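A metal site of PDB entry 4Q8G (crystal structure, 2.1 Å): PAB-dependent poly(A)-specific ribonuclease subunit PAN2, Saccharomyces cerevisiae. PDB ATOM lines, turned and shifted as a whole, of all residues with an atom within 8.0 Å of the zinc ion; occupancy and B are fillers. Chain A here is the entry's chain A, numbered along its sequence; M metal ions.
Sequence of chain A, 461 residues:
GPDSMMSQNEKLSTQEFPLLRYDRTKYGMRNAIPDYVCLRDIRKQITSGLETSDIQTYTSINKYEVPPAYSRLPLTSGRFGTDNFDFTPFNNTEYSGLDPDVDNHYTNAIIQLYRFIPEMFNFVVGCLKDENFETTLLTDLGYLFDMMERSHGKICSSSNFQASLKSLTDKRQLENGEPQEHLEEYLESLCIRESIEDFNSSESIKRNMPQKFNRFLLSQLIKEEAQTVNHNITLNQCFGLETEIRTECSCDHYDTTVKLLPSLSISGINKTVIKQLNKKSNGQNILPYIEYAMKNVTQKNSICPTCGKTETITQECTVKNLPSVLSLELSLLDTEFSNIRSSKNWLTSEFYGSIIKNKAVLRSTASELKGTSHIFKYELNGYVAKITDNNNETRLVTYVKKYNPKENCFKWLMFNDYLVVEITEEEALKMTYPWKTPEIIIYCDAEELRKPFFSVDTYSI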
ATOM      1  N   CYS A 249       0.711  21.984  27.558  1.00  0.00           N
ATOM      2  CA  CYS A 249       2.083  21.901  28.063  1.00  0.00           C
ATOM      3  C   CYS A 249       2.651  23.295  28.325  1.00  0.00           C
ATOM      4  O   CYS A 249       2.118  24.281  27.829  1.00  0.00           O
ATOM      5  CB  CYS A 249       2.938  21.190  27.035  1.00  0.00           C
ATOM      6  SG  CYS A 249       2.934  22.115  25.499  1.00  0.00           S
ATOM      7  N   SER A 250       3.765  23.394  29.042  1.00  0.00           N
ATOM      8  CA  SER A 250       4.359  24.700  29.372  1.00  0.00           C
ATOM      9  C   SER A 250       5.290  25.245  28.300  1.00  0.00           C
ATOM     10  O   SER A 250       5.654  26.405  28.356  1.00  0.00           O
ATOM     11  CB  SER A 250       5.150  24.630  30.685  1.00  0.00           C
ATOM     12  OG  SER A 250       4.495  23.820  31.646  1.00  0.00           O
ATOM     13  N   CYS A 251       5.710  24.424  27.347  1.00  0.00           N
ATOM     14  CA  CYS A 251       6.823  24.833  26.464  1.00  0.00           C
ATOM     15  C   CYS A 251       6.377  25.218  25.054  1.00  0.00           C
ATOM     16  O   CYS A 251       7.188  25.658  24.245  1.00  0.00           O
ATOM     17  CB  CYS A 251       7.869  23.717  26.388  1.00  0.00           C
ATOM     18  SG  CYS A 251       7.252  22.172  25.735  1.00  0.00           S
ATOM     19  N   ASP A 252       5.085  25.045  24.773  1.00  0.00           N
ATOM     20  CA  ASP A 252       4.483  25.502  23.507  1.00  0.00           C
ATOM     21  C   ASP A 252       4.855  24.636  22.297  1.00  0.00           C
ATOM     22  O   ASP A 252       4.667  25.043  21.148  1.00  0.00           O
ATOM     23  CB  ASP A 252       4.859  26.975  23.225  1.00  0.00           C
ATOM     24  CG  ASP A 252       3.994  27.621  22.150  1.00  0.00           C
ATOM     25  OD1 ASP A 252       2.890  27.108  21.839  1.00  0.00           O
ATOM     26  OD2 ASP A 252       4.415  28.686  21.629  1.00  0.00           O
ATOM     27  N   HIS A 253       5.339  23.425  22.540  1.00  0.00           N
ATOM     28  CA  HIS A 253       5.709  22.558  21.414  1.00  0.00           C
ATOM     29  C   HIS A 253       4.741  21.491  20.972  1.00  0.00           C
ATOM     30  O   HIS A 253       4.683  21.186  19.775  1.00  0.00           O
ATOM     31  CB  HIS A 253       7.032  21.895  21.749  1.00  0.00           C
ATOM     32  CG  HIS A 253       8.138  22.876  21.750  1.00  0.00           C
ATOM     33  ND1 HIS A 253       8.787  23.260  22.896  1.00  0.00           N
ATOM     34  CD2 HIS A 253       8.629  23.652  20.755  1.00  0.00           C
ATOM     35  CE1 HIS A 253       9.677  24.193  22.596  1.00  0.00           C
ATOM     36  NE2 HIS A 253       9.598  24.439  21.299  1.00  0.00           N
ATOM     37  N   TYR A 254       4.009  20.871  21.869  1.00  0.00           N
ATOM     38  CA  TYR A 254       3.476  19.548  21.509  1.00  0.00           C
ATOM     39  C   TYR A 254       2.342  19.707  20.484  1.00  0.00           C
ATOM     40  O   TYR A 254       1.160  19.649  20.842  1.00  0.00           O
ATOM     41  CB  TYR A 254       2.969  18.793  22.737  1.00  0.00           C
ATOM     42  CG  TYR A 254       3.996  18.162  23.656  1.00  0.00           C
ATOM     43  CD1 TYR A 254       4.237  16.788  23.637  1.00  0.00           C
ATOM     44  CD2 TYR A 254       4.680  18.926  24.603  1.00  0.00           C
ATOM     45  CE1 TYR A 254       5.155  16.199  24.501  1.00  0.00           C
ATOM     46  CE2 TYR A 254       5.586  18.365  25.466  1.00  0.00           C
ATOM     47  CZ  TYR A 254       5.813  17.002  25.430  1.00  0.00           C
ATOM     48  OH  TYR A 254       6.720  16.478  26.317  1.00  0.00           O
ATOM     49  N   ILE A 303       9.039  13.895  28.178  1.00  0.00           N
ATOM     50  CA  ILE A 303      10.201  14.694  27.770  1.00  0.00           C
ATOM     51  C   ILE A 303       9.885  15.260  26.399  1.00  0.00           C
ATOM     52  O   ILE A 303       9.578  14.505  25.474  1.00  0.00           O
ATOM     53  CB  ILE A 303      11.527  13.877  27.709  1.00  0.00           C
ATOM     54  CG1 ILE A 303      11.726  13.030  28.968  1.00  0.00           C
ATOM     55  CG2 ILE A 303      12.712  14.817  27.513  1.00  0.00           C
ATOM     56  CD1 ILE A 303      12.418  11.719  28.699  1.00  0.00           C
ATOM     57  N   CYS A 304       9.952  16.575  26.272  1.00  0.00           N
ATOM     58  CA  CYS A 304       9.650  17.218  25.007  1.00  0.00           C
ATOM     59  C   CYS A 304      10.747  16.925  23.986  1.00  0.00           C
ATOM     60  O   CYS A 304      11.912  17.246  24.232  1.00  0.00           O
ATOM     61  CB  CYS A 304       9.505  18.717  25.150  1.00  0.00           C
ATOM     62  SG  CYS A 304       8.975  19.498  23.600  1.00  0.00           S
ATOM     63  N   PRO A 305      10.376  16.381  22.834  1.00  0.00           N
ATOM     64  CA  PRO A 305      11.352  16.127  21.754  1.00  0.00           C
ATOM     65  C   PRO A 305      12.070  17.389  21.274  1.00  0.00           C
ATOM     66  O   PRO A 305      13.230  17.331  20.856  1.00  0.00           O
ATOM     67  CB  PRO A 305      10.493  15.536  20.655  1.00  0.00           C
ATOM     68  CG  PRO A 305       9.362  14.854  21.407  1.00  0.00           C
ATOM     69  CD  PRO A 305       9.057  15.803  22.529  1.00  0.00           C
ATOM     70  N   THR A 306      11.373  18.522  21.322  1.00  0.00           N
ATOM     71  CA  THR A 306      11.955  19.800  20.916  1.00  0.00           C
ATOM     72  C   THR A 306      12.753  20.482  22.034  1.00  0.00           C
ATOM     73  O   THR A 306      13.901  20.861  21.800  1.00  0.00           O
ATOM     74  CB  THR A 306      10.876  20.786  20.422  1.00  0.00           C
ATOM     75  OG1 THR A 306       9.882  20.078  19.675  1.00  0.00           O
ATOM     76  CG2 THR A 306      11.495  21.848  19.558  1.00  0.00           C
ATOM     77  N   CYS A 307      12.136  20.658  23.205  1.00  0.00           N
ATOM     78  CA  CYS A 307      12.766  21.336  24.362  1.00  0.00           C
ATOM     79  C   CYS A 307      13.740  20.423  25.071  1.00  0.00           C
ATOM     80  O   CYS A 307      14.837  20.835  25.408  1.00  0.00           O
ATOM     81  CB  CYS A 307      11.718  21.786  25.413  1.00  0.00           C
ATOM     82  SG  CYS A 307      11.176  23.463  25.297  1.00  0.00           S
ATOM     83  N   GLY A 308      13.295  19.202  25.364  1.00  0.00           N
ATOM     84  CA  GLY A 308      14.011  18.319  26.260  1.00  0.00           C
ATOM     85  C   GLY A 308      13.539  18.453  27.699  1.00  0.00           C
ATOM     86  O   GLY A 308      14.049  17.772  28.600  1.00  0.00           O
ATOM     87  N   LYS A 309      12.562  19.328  27.900  1.00  0.00           N
ATOM     88  CA  LYS A 309      12.010  19.567  29.232  1.00  0.00           C
ATOM     89  C   LYS A 309      11.175  18.381  29.662  1.00  0.00           C
ATOM     90  O   LYS A 309      10.416  17.849  28.878  1.00  0.00           O
ATOM     91  CB  LYS A 309      11.167  20.818  29.259  1.00  0.00           C
ATOM     92  N   THR A 310      11.343  17.972  30.908  1.00  0.00           N
ATOM     93  CA  THR A 310      10.521  16.935  31.486  1.00  0.00           C
ATOM     94  C   THR A 310       9.403  17.632  32.232  1.00  0.00           C
ATOM     95  O   THR A 310       9.629  18.626  32.916  1.00  0.00           O
ATOM     96  CB  THR A 310      11.295  16.002  32.403  1.00  0.00           C
ATOM     97  OG1 THR A 310      12.531  15.640  31.779  1.00  0.00           O
ATOM     98  CG2 THR A 310      10.508  14.751  32.667  1.00  0.00           C
ATOM     99  N   GLU A 311       8.187  17.122  32.038  1.00  0.00           N
ATOM    100  CA  GLU A 311       7.002  17.822  32.461  1.00  0.00           C
ATOM    101  C   GLU A 311       5.800  16.870  32.504  1.00  0.00           C
ATOM    102  O   GLU A 311       5.747  15.871  31.772  1.00  0.00           O
ATOM    103  CB  GLU A 311       6.734  18.984  31.504  1.00  0.00           C
ATOM    104  CG  GLU A 311       5.695  19.987  31.947  1.00  0.00           C
ATOM    105  CD  GLU A 311       5.177  20.827  30.781  1.00  0.00           C
ATOM    106  OE1 GLU A 311       5.847  20.910  29.728  1.00  0.00           O
ATOM    107  OE2 GLU A 311       4.079  21.401  30.908  1.00  0.00           O
HETATM  108 ZN    ZN M   1       9.190  21.627  24.429  1.00  0.00          ZN
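ND1 of His 253 sits close to SG of Cys 307, 3.4 Å away. The side-chain sulfur (SG) of Cys 304 sits close to the backbone NH (N) of Cys 307 (3.4 Å). The side-chain sulfur (SG) of Cys 304 lies close to the backbone NH (N) of Thr 306, at 3.4 Å. The backbone NH (N) of Cys 304 lies within hydrogen-bond range of the side-chain hydroxyl (OH) of Tyr 254. The backbone NH of Cys 304 sits at hydrogen-bond distance from the backbone carbonyl oxygen of Lys 309.
The nearest printed residue that does not touch the zinc ion is Thr 306 (4.4 Å).
The zinc ion is bound by a ring nitrogen (ND1) of His 253 (2.3 Å), the side-chain sulfur (SG) of Cys 304 (2.3 Å) and the side-chain sulfur (SG) of Cys 251 (2.4 Å). Slightly farther from the zinc ion lies SG of Cys 307 (2.8 Å).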
